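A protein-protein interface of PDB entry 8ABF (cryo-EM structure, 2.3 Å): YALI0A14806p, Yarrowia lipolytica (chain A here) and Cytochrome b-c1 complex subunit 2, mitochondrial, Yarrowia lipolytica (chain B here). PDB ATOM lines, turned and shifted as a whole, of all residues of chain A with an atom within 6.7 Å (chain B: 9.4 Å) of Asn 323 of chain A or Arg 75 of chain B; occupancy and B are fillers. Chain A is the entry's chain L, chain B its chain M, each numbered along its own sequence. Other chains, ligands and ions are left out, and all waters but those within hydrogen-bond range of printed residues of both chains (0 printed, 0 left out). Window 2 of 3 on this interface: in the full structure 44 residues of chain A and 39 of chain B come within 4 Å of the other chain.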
ATOM      1  N   TYR A 307     -22.487  16.571 -14.075  1.00  0.00           N
ATOM      2  CA  TYR A 307     -21.566  17.022 -13.063  1.00  0.00           C
ATOM      3  C   TYR A 307     -20.849  15.811 -12.501  1.00  0.00           C
ATOM      4  O   TYR A 307     -21.471  14.773 -12.350  1.00  0.00           O
ATOM      5  CB  TYR A 307     -22.364  17.671 -11.940  1.00  0.00           C
ATOM      6  CG  TYR A 307     -21.539  17.900 -10.710  1.00  0.00           C
ATOM      7  CD1 TYR A 307     -20.665  18.974 -10.661  1.00  0.00           C
ATOM      8  CD2 TYR A 307     -21.611  17.039  -9.623  1.00  0.00           C
ATOM      9  CE1 TYR A 307     -19.885  19.197  -9.542  1.00  0.00           C
ATOM     10  CE2 TYR A 307     -20.837  17.256  -8.491  1.00  0.00           C
ATOM     11  CZ  TYR A 307     -19.962  18.332  -8.464  1.00  0.00           C
ATOM     12  OH  TYR A 307     -19.194  18.592  -7.366  1.00  0.00           O
ATOM     13  N   SER A 314     -15.510  20.675 -13.055  1.00  0.00           N
ATOM     14  CA  SER A 314     -16.950  20.582 -12.838  1.00  0.00           C
ATOM     15  C   SER A 314     -17.425  21.604 -11.803  1.00  0.00           C
ATOM     16  O   SER A 314     -18.573  22.015 -11.832  1.00  0.00           O
ATOM     17  CB  SER A 314     -17.356  19.176 -12.491  1.00  0.00           C
ATOM     18  OG  SER A 314     -16.829  18.853 -11.219  1.00  0.00           O
ATOM     19  N   ARG A 315     -16.535  22.059 -10.918  1.00  0.00           N
ATOM     20  CA  ARG A 315     -16.930  23.059  -9.946  1.00  0.00           C
ATOM     21  C   ARG A 315     -17.138  24.418 -10.617  1.00  0.00           C
ATOM     22  O   ARG A 315     -17.713  25.307 -10.009  1.00  0.00           O
ATOM     23  CB  ARG A 315     -15.908  23.151  -8.816  1.00  0.00           C
ATOM     24  CG  ARG A 315     -14.697  23.988  -9.189  1.00  0.00           C
ATOM     25  CD  ARG A 315     -13.798  24.282  -8.011  1.00  0.00           C
ATOM     26  NE  ARG A 315     -13.227  23.039  -7.511  1.00  0.00           N
ATOM     27  CZ  ARG A 315     -13.403  22.539  -6.292  1.00  0.00           C
ATOM     28  NH1 ARG A 315     -14.110  23.192  -5.382  1.00  0.00           N
ATOM     29  NH2 ARG A 315     -12.833  21.389  -5.975  1.00  0.00           N
ATOM     30  N   HIS A 316     -16.720  24.575 -11.871  1.00  0.00           N
ATOM     31  CA  HIS A 316     -16.814  25.890 -12.479  1.00  0.00           C
ATOM     32  C   HIS A 316     -17.863  25.948 -13.577  1.00  0.00           C
ATOM     33  O   HIS A 316     -17.955  26.966 -14.253  1.00  0.00           O
ATOM     34  CB  HIS A 316     -15.472  26.287 -13.065  1.00  0.00           C
ATOM     35  CG  HIS A 316     -14.424  26.479 -12.036  1.00  0.00           C
ATOM     36  ND1 HIS A 316     -14.611  27.291 -10.937  1.00  0.00           N
ATOM     37  CD2 HIS A 316     -13.188  25.951 -11.924  1.00  0.00           C
ATOM     38  CE1 HIS A 316     -13.516  27.282 -10.199  1.00  0.00           C
ATOM     39  NE2 HIS A 316     -12.627  26.464 -10.787  1.00  0.00           N
ATOM     40  N   GLN A 317     -18.645  24.882 -13.751  1.00  0.00           N
ATOM     41  CA  GLN A 317     -19.625  24.848 -14.827  1.00  0.00           C
ATOM     42  C   GLN A 317     -20.715  25.893 -14.618  1.00  0.00           C
ATOM     43  O   GLN A 317     -21.044  26.267 -13.496  1.00  0.00           O
ATOM     44  CB  GLN A 317     -20.286  23.481 -14.910  1.00  0.00           C
ATOM     45  CG  GLN A 317     -19.307  22.396 -15.303  1.00  0.00           C
ATOM     46  CD  GLN A 317     -19.980  21.053 -15.430  1.00  0.00           C
ATOM     47  OE1 GLN A 317     -19.925  20.417 -16.480  1.00  0.00           O
ATOM     48  NE2 GLN A 317     -20.636  20.611 -14.369  1.00  0.00           N
ATOM     49  N   GLY A 318     -21.320  26.320 -15.727  1.00  0.00           N
ATOM     50  CA  GLY A 318     -22.325  27.373 -15.709  1.00  0.00           C
ATOM     51  C   GLY A 318     -23.712  26.941 -15.221  1.00  0.00           C
ATOM     52  O   GLY A 318     -24.483  27.779 -14.752  1.00  0.00           O
ATOM     53  N   SER A 319     -24.040  25.652 -15.357  1.00  0.00           N
ATOM     54  CA  SER A 319     -25.340  25.118 -14.972  1.00  0.00           C
ATOM     55  C   SER A 319     -25.662  25.471 -13.525  1.00  0.00           C
ATOM     56  O   SER A 319     -24.846  25.254 -12.634  1.00  0.00           O
ATOM     57  CB  SER A 319     -25.355  23.631 -15.203  1.00  0.00           C
ATOM     58  OG  SER A 319     -26.348  22.942 -14.438  1.00  0.00           O
ATOM     59  N   ARG A 320     -26.876  25.965 -13.293  1.00  0.00           N
ATOM     60  CA  ARG A 320     -27.317  26.289 -11.949  1.00  0.00           C
ATOM     61  C   ARG A 320     -27.294  25.074 -11.012  1.00  0.00           C
ATOM     62  O   ARG A 320     -26.860  25.179  -9.855  1.00  0.00           O
ATOM     63  CB  ARG A 320     -28.707  26.919 -12.013  1.00  0.00           C
ATOM     64  CG  ARG A 320     -29.274  27.237 -10.641  1.00  0.00           C
ATOM     65  CD  ARG A 320     -28.384  28.216  -9.892  1.00  0.00           C
ATOM     66  NE  ARG A 320     -28.927  28.579  -8.591  1.00  0.00           N
ATOM     67  CZ  ARG A 320     -28.229  29.080  -7.570  1.00  0.00           C
ATOM     68  NH1 ARG A 320     -26.912  29.178  -7.645  1.00  0.00           N
ATOM     69  NH2 ARG A 320     -28.845  29.382  -6.440  1.00  0.00           N
ATOM     70  N   LEU A 321     -27.792  23.928 -11.492  1.00  0.00           N
ATOM     71  CA  LEU A 321     -27.831  22.746 -10.642  1.00  0.00           C
ATOM     72  C   LEU A 321     -26.411  22.332 -10.282  1.00  0.00           C
ATOM     73  O   LEU A 321     -26.156  21.963  -9.140  1.00  0.00           O
ATOM     74  CB  LEU A 321     -28.583  21.586 -11.301  1.00  0.00           C
ATOM     75  CG  LEU A 321     -28.675  20.338 -10.421  1.00  0.00           C
ATOM     76  CD1 LEU A 321     -29.464  20.627  -9.148  1.00  0.00           C
ATOM     77  CD2 LEU A 321     -29.270  19.159 -11.172  1.00  0.00           C
ATOM     78  N   SER A 322     -25.492  22.432 -11.251  1.00  0.00           N
ATOM     79  CA  SER A 322     -24.090  22.138 -11.002  1.00  0.00           C
ATOM     80  C   SER A 322     -23.577  22.978  -9.830  1.00  0.00           C
ATOM     81  O   SER A 322     -22.936  22.449  -8.928  1.00  0.00           O
ATOM     82  CB  SER A 322     -23.272  22.378 -12.227  1.00  0.00           C
ATOM     83  OG  SER A 322     -21.930  21.995 -12.017  1.00  0.00           O
ATOM     84  N   ASN A 323     -23.890  24.274  -9.832  1.00  0.00           N
ATOM     85  CA  ASN A 323     -23.406  25.178  -8.803  1.00  0.00           C
ATOM     86  C   ASN A 323     -23.986  24.822  -7.447  1.00  0.00           C
ATOM     87  O   ASN A 323     -23.224  24.715  -6.494  1.00  0.00           O
ATOM     88  CB  ASN A 323     -23.701  26.625  -9.158  1.00  0.00           C
ATOM     89  CG  ASN A 323     -22.735  27.076 -10.224  1.00  0.00           C
ATOM     90  OD1 ASN A 323     -21.560  27.291  -9.936  1.00  0.00           O
ATOM     91  ND2 ASN A 323     -23.195  27.178 -11.460  1.00  0.00           N
ATOM     92  N   ILE A 324     -25.297  24.544  -7.392  1.00  0.00           N
ATOM     93  CA  ILE A 324     -25.949  24.183  -6.140  1.00  0.00           C
ATOM     94  C   ILE A 324     -25.318  22.916  -5.565  1.00  0.00           C
ATOM     95  O   ILE A 324     -25.025  22.831  -4.370  1.00  0.00           O
ATOM     96  CB  ILE A 324     -27.474  24.020  -6.322  1.00  0.00           C
ATOM     97  CG1 ILE A 324     -28.149  25.355  -6.657  1.00  0.00           C
ATOM     98  CG2 ILE A 324     -28.091  23.361  -5.088  1.00  0.00           C
ATOM     99  CD1 ILE A 324     -29.472  25.249  -7.413  1.00  0.00           C
ATOM    100  N   VAL A 325     -25.159  21.923  -6.431  1.00  0.00           N
ATOM    101  CA  VAL A 325     -24.725  20.612  -6.001  1.00  0.00           C
ATOM    102  C   VAL A 325     -23.276  20.671  -5.543  1.00  0.00           C
ATOM    103  O   VAL A 325     -22.945  20.103  -4.505  1.00  0.00           O
ATOM    104  CB  VAL A 325     -24.963  19.569  -7.104  1.00  0.00           C
ATOM    105  CG1 VAL A 325     -24.160  18.302  -6.873  1.00  0.00           C
ATOM    106  CG2 VAL A 325     -26.444  19.263  -7.199  1.00  0.00           C
ATOM    107  N   SER A 326     -22.430  21.365  -6.302  1.00  0.00           N
ATOM    108  CA  SER A 326     -21.028  21.395  -5.928  1.00  0.00           C
ATOM    109  C   SER A 326     -20.801  22.193  -4.646  1.00  0.00           C
ATOM    110  O   SER A 326     -20.095  21.705  -3.776  1.00  0.00           O
ATOM    111  CB  SER A 326     -20.138  21.827  -7.052  1.00  0.00           C
ATOM    112  OG  SER A 326     -20.478  23.141  -7.432  1.00  0.00           O
ATOM    113  N   GLU A 327     -21.438  23.365  -4.504  1.00  0.00           N
ATOM    114  CA  GLU A 327     -21.263  24.211  -3.323  1.00  0.00           C
ATOM    115  C   GLU A 327     -21.721  23.526  -2.033  1.00  0.00           C
ATOM    116  O   GLU A 327     -21.147  23.738  -0.965  1.00  0.00           O
ATOM    117  CB  GLU A 327     -22.036  25.521  -3.471  1.00  0.00           C
ATOM    118  CG  GLU A 327     -21.418  26.466  -4.479  1.00  0.00           C
ATOM    119  CD  GLU A 327     -22.225  27.731  -4.729  1.00  0.00           C
ATOM    120  OE1 GLU A 327     -23.373  27.630  -5.224  1.00  0.00           O
ATOM    121  OE2 GLU A 327     -21.706  28.822  -4.415  1.00  0.00           O
ATOM    122  N   ASN A 328     -22.741  22.682  -2.129  1.00  0.00           N
ATOM    123  CA  ASN A 328     -23.330  22.107  -0.943  1.00  0.00           C
ATOM    124  C   ASN A 328     -22.936  20.650  -0.771  1.00  0.00           C
ATOM    125  O   ASN A 328     -23.496  19.981   0.093  1.00  0.00           O
ATOM    126  CB  ASN A 328     -24.837  22.261  -1.038  1.00  0.00           C
ATOM    127  CG  ASN A 328     -25.194  23.722  -0.934  1.00  0.00           C
ATOM    128  OD1 ASN A 328     -25.036  24.323   0.123  1.00  0.00           O
ATOM    129  ND2 ASN A 328     -25.625  24.319  -2.028  1.00  0.00           N
ATOM    130  N   PHE A 334     -24.022  13.794 -11.274  1.00  0.00           N
ATOM    131  CA  PHE A 334     -25.319  13.645 -11.906  1.00  0.00           C
ATOM    132  C   PHE A 334     -25.117  13.698 -13.406  1.00  0.00           C
ATOM    133  O   PHE A 334     -24.168  14.318 -13.856  1.00  0.00           O
ATOM    134  CB  PHE A 334     -26.327  14.684 -11.410  1.00  0.00           C
ATOM    135  CG  PHE A 334     -26.052  16.142 -11.696  1.00  0.00           C
ATOM    136  CD1 PHE A 334     -26.245  16.679 -12.966  1.00  0.00           C
ATOM    137  CD2 PHE A 334     -25.673  17.002 -10.669  1.00  0.00           C
ATOM    138  CE1 PHE A 334     -26.059  18.033 -13.208  1.00  0.00           C
ATOM    139  CE2 PHE A 334     -25.481  18.357 -10.912  1.00  0.00           C
ATOM    140  CZ  PHE A 334     -25.672  18.870 -12.182  1.00  0.00           C
ATOM    141  N   ARG A 384     -26.654  29.693 -24.514  1.00  0.00           N
ATOM    142  CA  ARG A 384     -25.488  29.007 -23.985  1.00  0.00           C
ATOM    143  C   ARG A 384     -25.519  27.503 -24.286  1.00  0.00           C
ATOM    144  O   ARG A 384     -24.487  26.937 -24.637  1.00  0.00           O
ATOM    145  CB  ARG A 384     -25.373  29.271 -22.488  1.00  0.00           C
ATOM    146  CG  ARG A 384     -24.659  30.565 -22.116  1.00  0.00           C
ATOM    147  CD  ARG A 384     -24.363  30.674 -20.621  1.00  0.00           C
ATOM    148  NE  ARG A 384     -25.498  30.455 -19.726  1.00  0.00           N
ATOM    149  CZ  ARG A 384     -25.606  29.535 -18.763  1.00  0.00           C
ATOM    150  NH1 ARG A 384     -26.726  29.469 -18.064  1.00  0.00           N
ATOM    151  NH2 ARG A 384     -24.624  28.691 -18.493  1.00  0.00           N
ATOM    152  N   PHE B  62      -4.572  24.757 -16.207  1.00  0.00           N
ATOM    153  CA  PHE B  62      -5.871  25.400 -16.348  1.00  0.00           C
ATOM    154  C   PHE B  62      -6.461  25.764 -14.984  1.00  0.00           C
ATOM    155  O   PHE B  62      -7.674  25.863 -14.837  1.00  0.00           O
ATOM    156  CB  PHE B  62      -6.787  24.587 -17.265  1.00  0.00           C
ATOM    157  CG  PHE B  62      -6.237  24.442 -18.659  1.00  0.00           C
ATOM    158  CD1 PHE B  62      -6.298  25.504 -19.549  1.00  0.00           C
ATOM    159  CD2 PHE B  62      -5.611  23.273 -19.068  1.00  0.00           C
ATOM    160  CE1 PHE B  62      -5.773  25.397 -20.831  1.00  0.00           C
ATOM    161  CE2 PHE B  62      -5.065  23.173 -20.341  1.00  0.00           C
ATOM    162  CZ  PHE B  62      -5.156  24.227 -21.226  1.00  0.00           C
ATOM    163  N   LYS B  68      -6.377  35.035 -16.884  1.00  0.00           N
ATOM    164  CA  LYS B  68      -7.674  34.378 -16.972  1.00  0.00           C
ATOM    165  C   LYS B  68      -7.826  33.389 -15.825  1.00  0.00           C
ATOM    166  O   LYS B  68      -6.982  32.522 -15.652  1.00  0.00           O
ATOM    167  CB  LYS B  68      -7.783  33.651 -18.317  1.00  0.00           C
ATOM    168  CG  LYS B  68      -9.173  33.174 -18.715  1.00  0.00           C
ATOM    169  CD  LYS B  68      -9.177  32.311 -19.965  1.00  0.00           C
ATOM    170  CE  LYS B  68      -8.995  33.080 -21.258  1.00  0.00           C
ATOM    171  NZ  LYS B  68      -9.770  34.344 -21.274  1.00  0.00           N
ATOM    172  N   SER B  69      -8.912  33.511 -15.062  1.00  0.00           N
ATOM    173  CA  SER B  69      -9.136  32.625 -13.931  1.00  0.00           C
ATOM    174  C   SER B  69      -9.590  31.251 -14.415  1.00  0.00           C
ATOM    175  O   SER B  69     -10.091  31.113 -15.523  1.00  0.00           O
ATOM    176  CB  SER B  69     -10.149  33.213 -13.010  1.00  0.00           C
ATOM    177  OG  SER B  69     -11.423  33.238 -13.626  1.00  0.00           O
ATOM    178  N   ALA B  70      -9.425  30.237 -13.564  1.00  0.00           N
ATOM    179  CA  ALA B  70      -9.918  28.908 -13.889  1.00  0.00           C
ATOM    180  C   ALA B  70     -11.414  28.962 -14.220  1.00  0.00           C
ATOM    181  O   ALA B  70     -11.876  28.324 -15.165  1.00  0.00           O
ATOM    182  CB  ALA B  70      -9.616  27.963 -12.749  1.00  0.00           C
ATOM    183  N   LEU B  71     -12.156  29.766 -13.452  1.00  0.00           N
ATOM    184  CA  LEU B  71     -13.589  29.906 -13.623  1.00  0.00           C
ATOM    185  C   LEU B  71     -13.843  30.504 -14.991  1.00  0.00           C
ATOM    186  O   LEU B  71     -14.650  29.985 -15.740  1.00  0.00           O
ATOM    187  CB  LEU B  71     -14.127  30.842 -12.539  1.00  0.00           C
ATOM    188  CG  LEU B  71     -15.540  31.387 -12.753  1.00  0.00           C
ATOM    189  CD1 LEU B  71     -16.580  30.267 -12.750  1.00  0.00           C
ATOM    190  CD2 LEU B  71     -15.869  32.402 -11.666  1.00  0.00           C
ATOM    191  N   ARG B  72     -13.157  31.600 -15.302  1.00  0.00           N
ATOM    192  CA  ARG B  72     -13.452  32.213 -16.582  1.00  0.00           C
ATOM    193  C   ARG B  72     -13.106  31.278 -17.743  1.00  0.00           C
ATOM    194  O   ARG B  72     -13.796  31.278 -18.762  1.00  0.00           O
ATOM    195  CB  ARG B  72     -12.688  33.506 -16.782  1.00  0.00           C
ATOM    196  CG  ARG B  72     -13.069  34.087 -18.129  1.00  0.00           C
ATOM    197  CD  ARG B  72     -13.209  35.561 -18.290  1.00  0.00           C
ATOM    198  NE  ARG B  72     -13.640  36.328 -17.146  1.00  0.00           N
ATOM    199  CZ  ARG B  72     -14.582  37.256 -17.207  1.00  0.00           C
ATOM    200  NH1 ARG B  72     -15.223  37.481 -18.341  1.00  0.00           N
ATOM    201  NH2 ARG B  72     -14.886  37.935 -16.122  1.00  0.00           N
ATOM    202  N   PHE B  73     -12.016  30.519 -17.610  1.00  0.00           N
ATOM    203  CA  PHE B  73     -11.641  29.590 -18.657  1.00  0.00           C
ATOM    204  C   PHE B  73     -12.734  28.545 -18.885  1.00  0.00           C
ATOM    205  O   PHE B  73     -13.132  28.327 -20.021  1.00  0.00           O
ATOM    206  CB  PHE B  73     -10.300  28.939 -18.338  1.00  0.00           C
ATOM    207  CG  PHE B  73      -9.935  27.885 -19.349  1.00  0.00           C
ATOM    208  CD1 PHE B  73      -9.602  28.236 -20.653  1.00  0.00           C
ATOM    209  CD2 PHE B  73      -9.967  26.539 -19.014  1.00  0.00           C
ATOM    210  CE1 PHE B  73      -9.276  27.263 -21.592  1.00  0.00           C
ATOM    211  CE2 PHE B  73      -9.646  25.564 -19.952  1.00  0.00           C
ATOM    212  CZ  PHE B  73      -9.301  25.929 -21.240  1.00  0.00           C
ATOM    213  N   VAL B  74     -13.215  27.904 -17.816  1.00  0.00           N
ATOM    214  CA  VAL B  74     -14.245  26.882 -17.953  1.00  0.00           C
ATOM    215  C   VAL B  74     -15.519  27.468 -18.554  1.00  0.00           C
ATOM    216  O   VAL B  74     -16.159  26.817 -19.365  1.00  0.00           O
ATOM    217  CB  VAL B  74     -14.553  26.207 -16.606  1.00  0.00           C
ATOM    218  CG1 VAL B  74     -15.821  25.355 -16.650  1.00  0.00           C
ATOM    219  CG2 VAL B  74     -13.373  25.391 -16.138  1.00  0.00           C
ATOM    220  N   ARG B  75     -15.919  28.668 -18.134  1.00  0.00           N
ATOM    221  CA  ARG B  75     -17.157  29.213 -18.665  1.00  0.00           C
ATOM    222  C   ARG B  75     -17.009  29.528 -20.155  1.00  0.00           C
ATOM    223  O   ARG B  75     -17.970  29.427 -20.908  1.00  0.00           O
ATOM    224  CB  ARG B  75     -17.616  30.452 -17.894  1.00  0.00           C
ATOM    225  CG  ARG B  75     -18.015  30.199 -16.444  1.00  0.00           C
ATOM    226  CD  ARG B  75     -19.138  29.205 -16.229  1.00  0.00           C
ATOM    227  NE  ARG B  75     -19.448  29.133 -14.808  1.00  0.00           N
ATOM    228  CZ  ARG B  75     -20.337  29.900 -14.183  1.00  0.00           C
ATOM    229  NH1 ARG B  75     -21.022  30.816 -14.846  1.00  0.00           N
ATOM    230  NH2 ARG B  75     -20.522  29.754 -12.886  1.00  0.00           N
ATOM    231  N   GLU B  76     -15.810  29.913 -20.590  1.00  0.00           N
ATOM    232  CA  GLU B  76     -15.650  30.261 -21.994  1.00  0.00           C
ATOM    233  C   GLU B  76     -15.479  29.006 -22.836  1.00  0.00           C
ATOM    234  O   GLU B  76     -15.940  28.955 -23.970  1.00  0.00           O
ATOM    235  CB  GLU B  76     -14.453  31.172 -22.200  1.00  0.00           C
ATOM    236  CG  GLU B  76     -14.694  32.571 -21.694  1.00  0.00           C
ATOM    237  CD  GLU B  76     -13.484  33.487 -21.793  1.00  0.00           C
ATOM    238  OE1 GLU B  76     -13.669  34.726 -21.741  1.00  0.00           O
ATOM    239  OE2 GLU B  76     -12.352  32.966 -21.917  1.00  0.00           O
ATOM    240  N   LEU B  77     -14.794  28.003 -22.285  1.00  0.00           N
ATOM    241  CA  LEU B  77     -14.668  26.704 -22.927  1.00  0.00           C
ATOM    242  C   LEU B  77     -16.043  26.098 -23.230  1.00  0.00           C
ATOM    243  O   LEU B  77     -16.200  25.440 -24.255  1.00  0.00           O
ATOM    244  CB  LEU B  77     -13.855  25.812 -21.989  1.00  0.00           C
ATOM    245  CG  LEU B  77     -13.633  24.369 -22.431  1.00  0.00           C
ATOM    246  CD1 LEU B  77     -12.431  24.259 -23.361  1.00  0.00           C
ATOM    247  CD2 LEU B  77     -13.437  23.482 -21.216  1.00  0.00           C
ATOM    248  N   GLU B  78     -17.026  26.307 -22.337  1.00  0.00           N
ATOM    249  CA  GLU B  78     -18.378  25.796 -22.535  1.00  0.00           C
ATOM    250  C   GLU B  78     -19.074  26.526 -23.677  1.00  0.00           C
ATOM    251  O   GLU B  78     -19.871  25.914 -24.382  1.00  0.00           O
ATOM    252  CB  GLU B  78     -19.259  25.973 -21.298  1.00  0.00           C
ATOM    253  CG  GLU B  78     -18.909  25.068 -20.128  1.00  0.00           C
ATOM    254  CD  GLU B  78     -19.670  25.353 -18.833  1.00  0.00           C
ATOM    255  OE1 GLU B  78     -20.453  24.482 -18.377  1.00  0.00           O
ATOM    256  OE2 GLU B  78     -19.434  26.442 -18.257  1.00  0.00           O
ATOM    257  N   LEU B  79     -18.758  27.808 -23.879  1.00  0.00           N
ATOM    258  CA  LEU B  79     -19.326  28.557 -24.991  1.00  0.00           C
ATOM    259  C   LEU B  79     -18.788  28.103 -26.341  1.00  0.00           C
ATOM    260  O   LEU B  79     -19.429  28.341 -27.364  1.00  0.00           O
ATOM    261  CB  LEU B  79     -18.983  30.027 -24.815  1.00  0.00           C
ATOM    262  CG  LEU B  79     -19.710  30.693 -23.662  1.00  0.00           C
ATOM    263  CD1 LEU B  79     -19.330  32.156 -23.576  1.00  0.00           C
ATOM    264  CD2 LEU B  79     -21.218  30.522 -23.771  1.00  0.00           C
ATOM    265  N   PHE B  80     -17.578  27.536 -26.357  1.00  0.00           N
ATOM    266  CA  PHE B  80     -16.990  26.997 -27.572  1.00  0.00           C
ATOM    267  C   PHE B  80     -17.349  25.520 -27.702  1.00  0.00           C
ATOM    268  O   PHE B  80     -17.024  24.875 -28.701  1.00  0.00           O
ATOM    269  CB  PHE B  80     -15.470  27.104 -27.481  1.00  0.00           C
ATOM    270  CG  PHE B  80     -14.871  28.420 -27.905  1.00  0.00           C
ATOM    271  CD1 PHE B  80     -15.198  28.989 -29.127  1.00  0.00           C
ATOM    272  CD2 PHE B  80     -13.959  29.081 -27.094  1.00  0.00           C
ATOM    273  CE1 PHE B  80     -14.622  30.178 -29.544  1.00  0.00           C
ATOM    274  CE2 PHE B  80     -13.417  30.294 -27.490  1.00  0.00           C
ATOM    275  CZ  PHE B  80     -13.736  30.838 -28.718  1.00  0.00           C
ATOM    276  N   GLY B  81     -17.939  24.972 -26.638  1.00  0.00           N
ATOM    277  CA  GLY B  81     -18.204  23.546 -26.553  1.00  0.00           C
ATOM    278  C   GLY B  81     -16.931  22.702 -26.570  1.00  0.00           C
ATOM    279  O   GLY B  81     -16.996  21.519 -26.888  1.00  0.00           O
ATOM    280  N   GLY B  82     -15.780  23.302 -26.236  1.00  0.00           N
ATOM    281  CA  GLY B  82     -14.533  22.546 -26.190  1.00  0.00           C
ATOM    282  C   GLY B  82     -14.474  21.585 -25.001  1.00  0.00           C
ATOM    283  O   GLY B  82     -15.271  21.699 -24.076  1.00  0.00           O
ATOM    284  N   TYR B 106      -7.944  30.683 -29.864  1.00  0.00           N
ATOM    285  CA  TYR B 106      -8.280  30.729 -28.454  1.00  0.00           C
ATOM    286  C   TYR B 106      -7.487  29.668 -27.681  1.00  0.00           C
ATOM    287  O   TYR B 106      -6.955  29.941 -26.607  1.00  0.00           O
ATOM    288  CB  TYR B 106      -9.794  30.628 -28.276  1.00  0.00           C
ATOM    289  CG  TYR B 106     -10.187  30.623 -26.826  1.00  0.00           C
ATOM    290  CD1 TYR B 106     -10.218  29.435 -26.106  1.00  0.00           C
ATOM    291  CD2 TYR B 106     -10.472  31.812 -26.168  1.00  0.00           C
ATOM    292  CE1 TYR B 106     -10.540  29.438 -24.758  1.00  0.00           C
ATOM    293  CE2 TYR B 106     -10.806  31.827 -24.826  1.00  0.00           C
ATOM    294  CZ  TYR B 106     -10.843  30.634 -24.126  1.00  0.00           C
ATOM    295  OH  TYR B 106     -11.149  30.673 -22.802  1.00  0.00           O
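The backbone carbonyl oxygen of His 316 of chain A is in hydrogen-bond range of the guanidinium group of Arg 75 of chain B (2.7 Å).
The side-chain carboxylate (OE2) of Glu 78 of chain B is in hydrogen-bond range of the backbone NH (N) of Gly 318 of chain A, at 3.2 Å.
NE2 of Gln 317 of chain A lies within hydrogen-bond range of OG of Ser 322 of chain A (3.0 Å).
The side-chain amide nitrogen (ND2) of Asn 323 of chain A lies within hydrogen-bond range of the backbone carbonyl oxygen (O) of Gln 317 of chain A.
The side-chain amide nitrogen of Asn 323 of chain A lies within hydrogen-bond range of the backbone carbonyl oxygen of Ser 319 of chain A, 2.8 Å away.
The side-chain hydroxyl (OG) of Ser 326 of chain A lies within hydrogen-bond range of the backbone carbonyl oxygen (O) of Asn 323 of chain A (3.3 Å).
Ala 70 of chain B touches His 316 of chain A (CB to NE2, 3.9 Å).
His 316 of chain A touches Leu 71 of chain B (CG to CA, 3.9 Å).
O of His 316 of chain A touches CG1 of Val 74 of chain B, at 3.6 Å.
C of Gln 317 of chain A touches NE of Arg 75 of chain B, at 3.5 Å.
Gln 317 of chain A touches Glu 78 of chain B (CB to OE1, 3.6 Å).
Arg 75 of chain B touches Gly 318 of chain A (NE to CA, 3.5 Å).
ND2 of Asn 323 of chain A touches NH2 of Arg 75 of chain B, at 3.98 Å.
Leu 79 of chain B touches Arg 384 of chain A.
Of chain B, only Arg 75 comes within 4 Å of Asn 323 of chain A.
Arg 75 of chain B touches just these residues of chain A: His 316, Gln 317, Gly 318 and Asn 323.
Gly 318 of chain A touches just these residues of chain B: Arg 75 and Glu 78.
No residue of chain B comes within 4 Å of Ser 322 of chain A.
No residue of chain B comes within 4 Å of Ser 326 of chain A.
Of the printed residues of chain B, Gln 317 of chain A touches Arg 75 (3.5 Å) and Glu 78 (3.6 Å).
Of the printed residues of chain A, Ala 70 of chain B touches His 316 (3.9 Å).
The nearest residue of chain B that does not touch Asn 323 of chain A is Leu 71 of chain B (6.4 Å).
The nearest residue of chain A that does not touch Arg 75 of chain B is Arg 384 of chain A (5.5 Å).
Printed residues of chain A that touch a printed residue of chain B: His 316, Gln 317, Gly 318, Asn 323 and Arg 384.
Of the 17 printed residues of chain B, 6 touch a printed residue of chain A.
Hydrophobic or aromatic side chains of chain B within 4 Å of the printed part of chain A: Ala 70, Leu 71, Val 74 and Leu 79.
Among the printed residues, 10 pairs touch across the chains.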
